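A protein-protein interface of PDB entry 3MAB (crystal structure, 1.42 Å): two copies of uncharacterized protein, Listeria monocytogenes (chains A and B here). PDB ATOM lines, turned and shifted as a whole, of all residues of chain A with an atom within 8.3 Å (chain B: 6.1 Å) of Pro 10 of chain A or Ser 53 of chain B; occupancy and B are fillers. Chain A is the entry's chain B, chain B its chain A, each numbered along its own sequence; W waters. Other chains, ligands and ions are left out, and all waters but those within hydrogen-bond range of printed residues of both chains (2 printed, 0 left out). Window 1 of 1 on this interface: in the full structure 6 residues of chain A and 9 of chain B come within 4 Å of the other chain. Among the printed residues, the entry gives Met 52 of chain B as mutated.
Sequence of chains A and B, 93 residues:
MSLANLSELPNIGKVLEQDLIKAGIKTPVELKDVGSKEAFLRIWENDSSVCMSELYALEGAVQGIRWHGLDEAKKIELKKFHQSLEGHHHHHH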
ATOM      1  N   ASN A   5     -17.039  17.675 -27.784  1.00  0.00           N
ATOM      2  CA  ASN A   5     -15.962  17.577 -28.768  1.00  0.00           C
ATOM      3  C   ASN A   5     -15.544  16.118 -28.844  1.00  0.00           C
ATOM      4  O   ASN A   5     -15.650  15.389 -27.855  1.00  0.00           O
ATOM      5  CB  ASN A   5     -14.718  18.386 -28.341  1.00  0.00           C
ATOM      6  CG  ASN A   5     -14.867  19.854 -28.572  1.00  0.00           C
ATOM      7  OD1 ASN A   5     -15.316  20.282 -29.625  1.00  0.00           O
ATOM      8  ND2 ASN A   5     -14.478  20.645 -27.578  1.00  0.00           N
ATOM      9  N   LEU A   6     -15.001  15.680 -29.985  1.00  0.00           N
ATOM     10  CA  LEU A   6     -14.402  14.338 -30.095  1.00  0.00           C
ATOM     11  C   LEU A   6     -13.391  13.974 -29.028  1.00  0.00           C
ATOM     12  O   LEU A   6     -13.377  12.841 -28.524  1.00  0.00           O
ATOM     13  CB  LEU A   6     -13.795  14.126 -31.481  1.00  0.00           C
ATOM     14  CG  LEU A   6     -14.770  13.939 -32.632  1.00  0.00           C
ATOM     15  CD1 LEU A   6     -13.958  14.130 -33.956  1.00  0.00           C
ATOM     16  CD2 LEU A   6     -15.406  12.581 -32.592  1.00  0.00           C
ATOM     17  N   SER A   7     -12.530  14.926 -28.674  1.00  0.00           N
ATOM     18  CA  SER A   7     -11.505  14.668 -27.673  1.00  0.00           C
ATOM     19  C   SER A   7     -12.086  14.647 -26.252  1.00  0.00           C
ATOM     20  O   SER A   7     -11.321  14.450 -25.327  1.00  0.00           O
ATOM     21  CB  SER A   7     -10.397  15.712 -27.777  1.00  0.00           C
ATOM     22  OG  SER A   7     -10.898  16.991 -27.507  1.00  0.00           O
ATOM     23  N   GLU A   8     -13.388  14.905 -26.071  1.00  0.00           N
ATOM     24  CA  GLU A   8     -14.036  14.680 -24.769  1.00  0.00           C
ATOM     25  C   GLU A   8     -14.642  13.268 -24.644  1.00  0.00           C
ATOM     26  O   GLU A   8     -15.080  12.880 -23.562  1.00  0.00           O
ATOM     27  CB  GLU A   8     -15.132  15.689 -24.487  1.00  0.00           C
ATOM     28  CG  GLU A   8     -14.588  17.111 -24.318  1.00  0.00           C
ATOM     29  CD  GLU A   8     -15.670  18.172 -24.247  1.00  0.00           C
ATOM     30  OE1 GLU A   8     -16.493  18.235 -25.183  1.00  0.00           O
ATOM     31  OE2 GLU A   8     -15.655  19.010 -23.296  1.00  0.00           O
ATOM     32  N   LEU A   9     -14.675  12.532 -25.738  1.00  0.00           N
ATOM     33  CA  LEU A   9     -15.148  11.141 -25.684  1.00  0.00           C
ATOM     34  C   LEU A   9     -14.098  10.215 -25.114  1.00  0.00           C
ATOM     35  O   LEU A   9     -12.878  10.447 -25.256  1.00  0.00           O
ATOM     36  CB  LEU A   9     -15.483  10.628 -27.049  1.00  0.00           C
ATOM     37  CG  LEU A   9     -16.499  11.427 -27.840  1.00  0.00           C
ATOM     38  CD1 LEU A   9     -16.695  10.783 -29.195  1.00  0.00           C
ATOM     39  CD2 LEU A   9     -17.855  11.690 -27.145  1.00  0.00           C
ATOM     40  N   PRO A  10     -14.549   9.122 -24.462  1.00  0.00           N
ATOM     41  CA  PRO A  10     -13.552   8.164 -23.932  1.00  0.00           C
ATOM     42  C   PRO A  10     -12.575   7.687 -25.024  1.00  0.00           C
ATOM     43  O   PRO A  10     -13.006   7.420 -26.170  1.00  0.00           O
ATOM     44  CB  PRO A  10     -14.403   6.998 -23.417  1.00  0.00           C
ATOM     45  CG  PRO A  10     -15.802   7.465 -23.503  1.00  0.00           C
ATOM     46  CD  PRO A  10     -15.933   8.664 -24.280  1.00  0.00           C
ATOM     47  N   ASN A  11     -11.296   7.542 -24.682  1.00  0.00           N
ATOM     48  CA  ASN A  11     -10.218   7.021 -25.524  1.00  0.00           C
ATOM     49  C   ASN A  11      -9.726   7.886 -26.650  1.00  0.00           C
ATOM     50  O   ASN A  11      -8.795   7.468 -27.327  1.00  0.00           O
ATOM     51  CB  ASN A  11     -10.624   5.650 -26.120  1.00  0.00           C
ATOM     52  CG  ASN A  11     -11.382   4.799 -25.136  1.00  0.00           C
ATOM     53  OD1 ASN A  11     -10.850   4.457 -24.091  1.00  0.00           O
ATOM     54  ND2 ASN A  11     -12.646   4.492 -25.446  1.00  0.00           N
ATOM     55  N   ILE A  12     -10.359   9.019 -26.903  1.00  0.00           N
ATOM     56  CA  ILE A  12      -9.958   9.877 -28.021  1.00  0.00           C
ATOM     57  C   ILE A  12      -9.007  10.961 -27.582  1.00  0.00           C
ATOM     58  O   ILE A  12      -9.461  11.926 -26.993  1.00  0.00           O
ATOM     59  CB  ILE A  12     -11.179  10.461 -28.767  1.00  0.00           C
ATOM     60  CG1 ILE A  12     -12.105   9.321 -29.164  1.00  0.00           C
ATOM     61  CG2 ILE A  12     -10.669  11.242 -30.016  1.00  0.00           C
ATOM     62  CD1 ILE A  12     -13.190   9.651 -30.161  1.00  0.00           C
ATOM     63  N   GLY A  13      -7.709  10.775 -27.873  1.00  0.00           N
ATOM     64  CA  GLY A  13      -6.688  11.787 -27.641  1.00  0.00           C
ATOM     65  C   GLY A  13      -6.681  12.838 -28.712  1.00  0.00           C
ATOM     66  O   GLY A  13      -7.399  12.759 -29.695  1.00  0.00           O
ATOM     67  N   LEU A  16      -5.715  11.492 -32.322  1.00  0.00           N
ATOM     68  CA  LEU A  16      -6.804  10.733 -32.936  1.00  0.00           C
ATOM     69  C   LEU A  16      -7.992  11.647 -33.331  1.00  0.00           C
ATOM     70  O   LEU A  16      -8.593  11.436 -34.377  1.00  0.00           O
ATOM     71  CB  LEU A  16      -7.268   9.614 -32.002  1.00  0.00           C
ATOM     72  CG  LEU A  16      -8.361   8.678 -32.474  1.00  0.00           C
ATOM     73  CD1 LEU A  16      -8.065   8.072 -33.885  1.00  0.00           C
ATOM     74  CD2 LEU A  16      -8.603   7.555 -31.465  1.00  0.00           C
ATOM     75  N   PRO A  28     -18.803  13.966 -32.258  1.00  0.00           N
ATOM     76  CA  PRO A  28     -19.246  12.681 -31.744  1.00  0.00           C
ATOM     77  C   PRO A  28     -20.431  12.080 -32.479  1.00  0.00           C
ATOM     78  O   PRO A  28     -20.491  10.866 -32.610  1.00  0.00           O
ATOM     79  CB  PRO A  28     -19.622  13.009 -30.281  1.00  0.00           C
ATOM     80  CG  PRO A  28     -18.662  14.132 -29.954  1.00  0.00           C
ATOM     81  CD  PRO A  28     -18.568  14.946 -31.162  1.00  0.00           C
ATOM     82  N   LEU A  31     -19.188  10.462 -35.622  1.00  0.00           N
ATOM     83  CA  LEU A  31     -18.543   9.203 -35.288  1.00  0.00           C
ATOM     84  C   LEU A  31     -19.526   8.096 -35.007  1.00  0.00           C
ATOM     85  O   LEU A  31     -19.357   6.986 -35.519  1.00  0.00           O
ATOM     86  CB  LEU A  31     -17.536   9.334 -34.151  1.00  0.00           C
ATOM     87  CG  LEU A  31     -16.849   8.085 -33.631  1.00  0.00           C
ATOM     88  CD1 LEU A  31     -16.021   7.436 -34.664  1.00  0.00           C
ATOM     89  CD2 LEU A  31     -15.990   8.417 -32.424  1.00  0.00           C
ATOM     90  N   TYR A  56      -9.977  -0.151 -31.150  1.00  0.00           N
ATOM     91  CA  TYR A  56     -10.565  -0.267 -29.830  1.00  0.00           C
ATOM     92  C   TYR A  56     -10.991   1.076 -29.278  1.00  0.00           C
ATOM     93  O   TYR A  56     -12.095   1.178 -28.690  1.00  0.00           O
ATOM     94  CB  TYR A  56      -9.579  -0.938 -28.865  1.00  0.00           C
ATOM     95  CG  TYR A  56      -9.419  -2.454 -28.909  1.00  0.00           C
ATOM     96  CD1 TYR A  56     -10.297  -3.273 -29.572  1.00  0.00           C
ATOM     97  CD2 TYR A  56      -8.406  -3.043 -28.185  1.00  0.00           C
ATOM     98  CE1 TYR A  56     -10.117  -4.677 -29.606  1.00  0.00           C
ATOM     99  CE2 TYR A  56      -8.235  -4.461 -28.228  1.00  0.00           C
ATOM    100  CZ  TYR A  56      -9.114  -5.213 -28.915  1.00  0.00           C
ATOM    101  OH  TYR A  56      -8.909  -6.575 -28.880  1.00  0.00           O
ATOM    102  N   ALA A  57     -10.145   2.104 -29.406  1.00  0.00           N
ATOM    103  CA  ALA A  57     -10.477   3.440 -28.914  1.00  0.00           C
ATOM    104  C   ALA A  57     -11.736   3.984 -29.525  1.00  0.00           C
ATOM    105  O   ALA A  57     -12.599   4.530 -28.842  1.00  0.00           O
ATOM    106  CB  ALA A  57      -9.309   4.415 -29.171  1.00  0.00           C
ATOM    107  N   LEU A  58     -11.880   3.792 -30.825  1.00  0.00           N
ATOM    108  CA  LEU A  58     -13.007   4.281 -31.563  1.00  0.00           C
ATOM    109  C   LEU A  58     -14.292   3.561 -31.150  1.00  0.00           C
ATOM    110  O   LEU A  58     -15.333   4.189 -30.964  1.00  0.00           O
ATOM    111  CB  LEU A  58     -12.798   4.153 -33.069  1.00  0.00           C
ATOM    112  CG  LEU A  58     -11.752   5.068 -33.621  1.00  0.00           C
ATOM    113  CD1 LEU A  58     -11.443   4.688 -35.056  1.00  0.00           C
ATOM    114  CD2 LEU A  58     -12.169   6.518 -33.623  1.00  0.00           C
ATOM    115  N   GLU A  59     -14.243   2.227 -30.985  1.00  0.00           N
ATOM    116  CA  GLU A  59     -15.442   1.502 -30.557  1.00  0.00           C
ATOM    117  C   GLU A  59     -15.821   1.870 -29.157  1.00  0.00           C
ATOM    118  O   GLU A  59     -17.002   2.052 -28.850  1.00  0.00           O
ATOM    119  CB  GLU A  59     -15.253  -0.021 -30.667  1.00  0.00           C
ATOM    120  CG  GLU A  59     -16.430  -0.864 -30.273  1.00  0.00           C
ATOM    121  CD  GLU A  59     -17.659  -0.667 -31.132  1.00  0.00           C
ATOM    122  OE1 GLU A  59     -17.499  -0.291 -32.306  1.00  0.00           O
ATOM    123  OE2 GLU A  59     -18.794  -0.956 -30.681  1.00  0.00           O
ATOM    124  N   GLY A  60     -14.831   2.009 -28.270  1.00  0.00           N
ATOM    125  CA  GLY A  60     -15.102   2.441 -26.919  1.00  0.00           C
ATOM    126  C   GLY A  60     -15.726   3.849 -26.938  1.00  0.00           C
ATOM    127  O   GLY A  60     -16.691   4.109 -26.229  1.00  0.00           O
ATOM    128  N   ALA A  61     -15.226   4.726 -27.769  1.00  0.00           N
ATOM    129  CA  ALA A  61     -15.831   6.072 -27.885  1.00  0.00           C
ATOM    130  C   ALA A  61     -17.305   6.005 -28.287  1.00  0.00           C
ATOM    131  O   ALA A  61     -18.161   6.671 -27.676  1.00  0.00           O
ATOM    132  CB  ALA A  61     -15.022   6.943 -28.857  1.00  0.00           C
ATOM    133  N   VAL A  62     -17.598   5.196 -29.296  1.00  0.00           N
ATOM    134  CA  VAL A  62     -18.961   4.989 -29.779  1.00  0.00           C
ATOM    135  C   VAL A  62     -19.876   4.475 -28.677  1.00  0.00           C
ATOM    136  O   VAL A  62     -21.033   4.931 -28.528  1.00  0.00           O
ATOM    137  CB  VAL A  62     -18.972   4.060 -31.018  1.00  0.00           C
ATOM    138  CG1 VAL A  62     -20.401   3.623 -31.388  1.00  0.00           C
ATOM    139  CG2 VAL A  62     -18.256   4.764 -32.237  1.00  0.00           C
ATOM    140  N   GLN A  63     -19.359   3.554 -27.872  1.00  0.00           N
ATOM    141  CA  GLN A  63     -20.121   2.953 -26.779  1.00  0.00           C
ATOM    142  C   GLN A  63     -20.132   3.778 -25.548  1.00  0.00           C
ATOM    143  O   GLN A  63     -20.831   3.440 -24.584  1.00  0.00           O
ATOM    144  CB  GLN A  63     -19.592   1.540 -26.464  1.00  0.00           C
ATOM    145  CG  GLN A  63     -19.905   0.595 -27.553  1.00  0.00           C
ATOM    146  CD  GLN A  63     -19.721  -0.846 -27.135  1.00  0.00           C
ATOM    147  OE1 GLN A  63     -19.942  -1.167 -25.948  1.00  0.00           O
ATOM    148  NE2 GLN A  63     -19.349  -1.718 -28.060  1.00  0.00           N
ATOM    149  N   GLY A  64     -19.359   4.864 -25.498  1.00  0.00           N
ATOM    150  CA  GLY A  64     -19.261   5.653 -24.292  1.00  0.00           C
ATOM    151  C   GLY A  64     -18.525   5.044 -23.105  1.00  0.00           C
ATOM    152  O   GLY A  64     -18.810   5.354 -21.931  1.00  0.00           O
ATOM    153  N   ILE A  65     -17.502   4.241 -23.391  1.00  0.00           N
ATOM    154  CA  ILE A  65     -16.735   3.543 -22.361  1.00  0.00           C
ATOM    155  C   ILE A  65     -15.247   3.524 -22.637  1.00  0.00           C
ATOM    156  O   ILE A  65     -14.871   3.538 -23.804  1.00  0.00           O
ATOM    157  CB  ILE A  65     -17.218   2.084 -22.146  1.00  0.00           C
ATOM    158  CG1 ILE A  65     -16.999   1.238 -23.381  1.00  0.00           C
ATOM    159  CG2 ILE A  65     -18.691   2.035 -21.753  1.00  0.00           C
ATOM    160  CD1 ILE A  65     -17.341  -0.283 -23.197  1.00  0.00           C
ATOM    161  N   ARG A  66     -14.397   3.432 -21.602  1.00  0.00           N
ATOM    162  CA  ARG A  66     -12.987   3.155 -21.822  1.00  0.00           C
ATOM    163  C   ARG A  66     -12.901   1.830 -22.556  1.00  0.00           C
ATOM    164  O   ARG A  66     -13.670   0.911 -22.278  1.00  0.00           O
ATOM    165  CB  ARG A  66     -12.097   3.209 -20.562  1.00  0.00           C
ATOM    166  CG  ARG A  66     -12.348   2.167 -19.524  1.00  0.00           C
ATOM    167  CD  ARG A  66     -11.546   2.596 -18.281  1.00  0.00           C
ATOM    168  NE  ARG A  66     -11.511   1.598 -17.238  1.00  0.00           N
ATOM    169  CZ  ARG A  66     -12.497   1.359 -16.381  1.00  0.00           C
ATOM    170  NH1 ARG A  66     -13.645   2.015 -16.460  1.00  0.00           N
ATOM    171  NH2 ARG A  66     -12.346   0.425 -15.455  1.00  0.00           N
ATOM    172  N   TRP A  67     -11.989   1.744 -23.516  1.00  0.00           N
ATOM    173  CA  TRP A  67     -11.908   0.578 -24.373  1.00  0.00           C
ATOM    174  C   TRP A  67     -11.616  -0.661 -23.557  1.00  0.00           C
ATOM    175  O   TRP A  67     -11.979  -1.739 -23.967  1.00  0.00           O
ATOM    176  CB  TRP A  67     -10.848   0.707 -25.531  1.00  0.00           C
ATOM    177  CG  TRP A  67      -9.447   0.901 -25.027  1.00  0.00           C
ATOM    178  CD1 TRP A  67      -8.796   2.089 -24.806  1.00  0.00           C
ATOM    179  CD2 TRP A  67      -8.546  -0.117 -24.637  1.00  0.00           C
ATOM    180  NE1 TRP A  67      -7.558   1.870 -24.240  1.00  0.00           N
ATOM    181  CE2 TRP A  67      -7.373   0.517 -24.134  1.00  0.00           C
ATOM    182  CE3 TRP A  67      -8.608  -1.519 -24.631  1.00  0.00           C
ATOM    183  CZ2 TRP A  67      -6.267  -0.200 -23.675  1.00  0.00           C
ATOM    184  CZ3 TRP A  67      -7.508  -2.236 -24.161  1.00  0.00           C
ATOM    185  CH2 TRP A  67      -6.343  -1.567 -23.689  1.00  0.00           C
ATOM    186  N   HIS A  68     -10.985  -0.459 -22.392  1.00  0.00           N
ATOM    187  CA  HIS A  68     -10.599  -1.561 -21.547  1.00  0.00           C
ATOM    188  C   HIS A  68     -11.875  -2.371 -21.179  1.00  0.00           C
ATOM    189  O   HIS A  68     -11.802  -3.573 -20.962  1.00  0.00           O
ATOM    190  CB  HIS A  68      -9.910  -1.081 -20.263  1.00  0.00           C
ATOM    191  CG  HIS A  68      -8.852  -0.021 -20.460  1.00  0.00           C
ATOM    192  ND1 HIS A  68      -9.149   1.239 -20.922  1.00  0.00           N
ATOM    193  CD2 HIS A  68      -7.530   0.004 -20.130  1.00  0.00           C
ATOM    194  CE1 HIS A  68      -8.046   1.982 -20.940  1.00  0.00           C
ATOM    195  NE2 HIS A  68      -7.052   1.262 -20.455  1.00  0.00           N
ATOM    196  N   CYS B  51     -11.041   7.198 -16.722  1.00  0.00           N
ATOM    197  CA  CYS B  51     -10.658   8.317 -17.555  1.00  0.00           C
ATOM    198  C   CYS B  51     -11.479   9.565 -17.344  1.00  0.00           C
ATOM    199  O   CYS B  51     -12.574   9.502 -16.747  1.00  0.00           O
ATOM    200  CB  CYS B  51     -10.702   7.871 -19.022  1.00  0.00           C
ATOM    201  SG  CYS B  51     -12.333   7.643 -19.784  1.00  0.00           S
ATOM    202  N   MET B  52     -10.972  10.689 -17.859  1.00  0.00           N
ATOM    203  CA  MET B  52     -11.659  11.977 -17.735  1.00  0.00           C
ATOM    204  C   MET B  52     -13.118  11.909 -18.180  1.00  0.00           C
ATOM    205  O   MET B  52     -14.033  12.438 -17.534  1.00  0.00           O
ATOM    206  CB  MET B  52     -10.945  13.062 -18.517  1.00  0.00           C
ATOM    207  CG  MET B  52     -11.676  14.391 -18.429  1.00  0.00           C
ATOM    208  SD  MET B  52     -11.541  15.143 -16.798  1.00  0.00           S
ATOM    209  CE  MET B  52     -13.229  15.477 -16.377  1.00  0.00           C
ATOM    210  N   SER B  53     -13.375  11.201 -19.254  1.00  0.00           N
ATOM    211  CA  SER B  53     -14.715  11.013 -19.738  1.00  0.00           C
ATOM    212  C   SER B  53     -15.620  10.310 -18.743  1.00  0.00           C
ATOM    213  O   SER B  53     -16.786  10.619 -18.698  1.00  0.00           O
ATOM    214  CB  SER B  53     -14.649  10.252 -21.070  1.00  0.00           C
ATOM    215  OG  SER B  53     -14.015  11.064 -22.016  1.00  0.00           O
ATOM    216  N   GLU B  54     -15.093   9.351 -17.983  1.00  0.00           N
ATOM    217  CA  GLU B  54     -15.871   8.632 -17.016  1.00  0.00           C
ATOM    218  C   GLU B  54     -16.162   9.500 -15.789  1.00  0.00           C
ATOM    219  O   GLU B  54     -17.232   9.402 -15.169  1.00  0.00           O
ATOM    220  CB  GLU B  54     -15.191   7.340 -16.652  1.00  0.00           C
ATOM    221  CG  GLU B  54     -15.323   6.328 -17.764  1.00  0.00           C
ATOM    222  CD  GLU B  54     -14.557   5.079 -17.478  1.00  0.00           C
ATOM    223  OE1 GLU B  54     -13.317   5.168 -17.526  1.00  0.00           O
ATOM    224  OE2 GLU B  54     -15.202   4.043 -17.152  1.00  0.00           O
ATOM    225  N   LEU B  55     -15.294  10.478 -15.465  1.00  0.00           N
ATOM    226  CA  LEU B  55     -15.628  11.502 -14.480  1.00  0.00           C
ATOM    227  C   LEU B  55     -16.823  12.352 -14.953  1.00  0.00           C
ATOM    228  O   LEU B  55     -17.756  12.598 -14.157  1.00  0.00           O
ATOM    229  CB  LEU B  55     -14.389  12.328 -14.168  1.00  0.00           C
ATOM    230  CG  LEU B  55     -14.563  13.508 -13.197  1.00  0.00           C
ATOM    231  CD1 LEU B  55     -15.110  13.082 -11.793  1.00  0.00           C
ATOM    232  CD2 LEU B  55     -13.284  14.241 -13.058  1.00  0.00           C
ATOM    233  N   TYR B  56     -16.848  12.777 -16.192  1.00  0.00           N
ATOM    234  CA  TYR B  56     -17.996  13.493 -16.747  1.00  0.00           C
ATOM    235  C   TYR B  56     -19.241  12.632 -16.658  1.00  0.00           C
ATOM    236  O   TYR B  56     -20.309  13.097 -16.221  1.00  0.00           O
ATOM    237  CB  TYR B  56     -17.796  13.845 -18.213  1.00  0.00           C
ATOM    238  CG  TYR B  56     -16.850  14.973 -18.511  1.00  0.00           C
ATOM    239  CD1 TYR B  56     -16.259  15.714 -17.518  1.00  0.00           C
ATOM    240  CD2 TYR B  56     -16.580  15.316 -19.787  1.00  0.00           C
ATOM    241  CE1 TYR B  56     -15.391  16.783 -17.827  1.00  0.00           C
ATOM    242  CE2 TYR B  56     -15.722  16.413 -20.109  1.00  0.00           C
ATOM    243  CZ  TYR B  56     -15.136  17.095 -19.102  1.00  0.00           C
ATOM    244  OH  TYR B  56     -14.293  18.224 -19.392  1.00  0.00           O
ATOM    245  N   ALA B  57     -19.133  11.331 -16.966  1.00  0.00           N
ATOM    246  CA  ALA B  57     -20.267  10.395 -16.876  1.00  0.00           C
ATOM    247  C   ALA B  57     -20.814  10.308 -15.465  1.00  0.00           C
ATOM    248  O   ALA B  57     -22.064  10.349 -15.288  1.00  0.00           O
ATOM    249  CB  ALA B  57     -19.805   8.981 -17.354  1.00  0.00           C
ATOM    250  N   LEU B  58     -19.950  10.217 -14.467  1.00  0.00           N
ATOM    251  CA  LEU B  58     -20.406  10.154 -13.091  1.00  0.00           C
ATOM    252  C   LEU B  58     -21.117  11.406 -12.675  1.00  0.00           C
ATOM    253  O   LEU B  58     -22.129  11.342 -12.006  1.00  0.00           O
ATOM    254  CB  LEU B  58     -19.225   9.884 -12.173  1.00  0.00           C
ATOM    255  CG  LEU B  58     -18.616   8.484 -12.293  1.00  0.00           C
ATOM    256  CD1 LEU B  58     -17.312   8.366 -11.600  1.00  0.00           C
ATOM    257  CD2 LEU B  58     -19.561   7.368 -11.871  1.00  0.00           C
ATOM    258  N   TRP B  67     -24.100  13.411 -20.032  1.00  0.00           N
ATOM    259  CA  TRP B  67     -23.024  14.290 -19.657  1.00  0.00           C
ATOM    260  C   TRP B  67     -22.677  15.383 -20.667  1.00  0.00           C
ATOM    261  O   TRP B  67     -22.154  16.422 -20.274  1.00  0.00           O
ATOM    262  CB  TRP B  67     -21.753  13.569 -19.212  1.00  0.00           C
ATOM    263  CG  TRP B  67     -20.963  12.872 -20.273  1.00  0.00           C
ATOM    264  CD1 TRP B  67     -20.922  11.526 -20.447  1.00  0.00           C
ATOM    265  CD2 TRP B  67     -20.043  13.434 -21.222  1.00  0.00           C
ATOM    266  NE1 TRP B  67     -20.067  11.212 -21.478  1.00  0.00           N
ATOM    267  CE2 TRP B  67     -19.508  12.363 -21.955  1.00  0.00           C
ATOM    268  CE3 TRP B  67     -19.641  14.728 -21.530  1.00  0.00           C
ATOM    269  CZ2 TRP B  67     -18.587  12.544 -23.002  1.00  0.00           C
ATOM    270  CZ3 TRP B  67     -18.703  14.923 -22.593  1.00  0.00           C
ATOM    271  CH2 TRP B  67     -18.213  13.828 -23.313  1.00  0.00           C
HETATM  272  O   HOH W   1      -9.861   8.439 -22.415  1.00  0.00           O
HETATM  273  O   HOH W   2     -13.197  18.847 -21.818  1.00  0.00           O
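Among the printed residues, pairs that only touch across the chains: Glu 8 of chain A with Trp 67 of chain B.
Printed residues of chain B that touch a printed residue of chain A: Ser 53, Glu 54 and Trp 67.
Of the 25 printed residues of chain A, 4 touch a printed residue of chain B.
Hydrophobic or aromatic side chains of chain A that line the printed part of chain B: Pro 10.
Along chain A the printed residues that touch a printed residue of chain B span positions 8 to 66.
Among the printed residues, Asp or Glu carboxylates within 4 Å of a Lys or Arg side-chain nitrogen of the other chain: Arg 66 of chain A with Glu 54 of chain B (2.6 Å).
The side-chain sulfur (SG) of Cys 51 of chain B sits close to the backbone NH (N) of Ser 53 of chain B.
OE1 of Glu 8 of chain A sits at hydrogen-bond distance from N of Asn 5 of chain A, at 2.7 Å.
N of Cys 51 of chain B lies within hydrogen-bond range of OE1 of Glu 54 of chain B, at 3.2 Å.
Positions printed for both chains: 56, 57, 58 and 67.
Water W2 bridges the side-chain hydroxyl (OH) of Tyr 56 of chain B (2.7 Å) and the side-chain carboxylate (OE2) of Glu 8 of chain A (2.9 Å).
Water W1 lies within hydrogen-bond range of the backbone NH (N) of Asn 11 of chain A (2.8 Å) and the side-chain sulfur (SG) of Cys 51 of chain B (3.7 Å).
O of Glu 8 of chain A sits at hydrogen-bond distance from OG of Ser 53 of chain B, 2.6 Å away.
The side-chain hydroxyl (OG) of Ser 53 of chain B sits close to the backbone carbonyl oxygen (O) of Leu 9 of chain A (3.5 Å).
The side-chain carboxylate of Glu 54 of chain B lies within salt-bridge range of the guanidinium group of Arg 66 of chain A (2.6 Å).
The side-chain hydroxyl (OG) of Ser 53 of chain B lies close to the backbone nitrogen (N) of Pro 10 of chain A (3.2 Å).
Of the printed residues of chain A, Ser 53 of chain B touches Glu 8, Leu 9 and Pro 10.
Printed residues of chain B within 4 Å of Arg 66 of chain A: Glu 54 (2.6 Å).
Printed residues of chain A within 4 Å of Trp 67 of chain B: Glu 8.
Val 62 of chain A touches none of the printed residues of chain B.
The nearest printed residue of chain A that does not touch Ser 53 of chain B is Asn 11 of chain A (5.2 Å).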
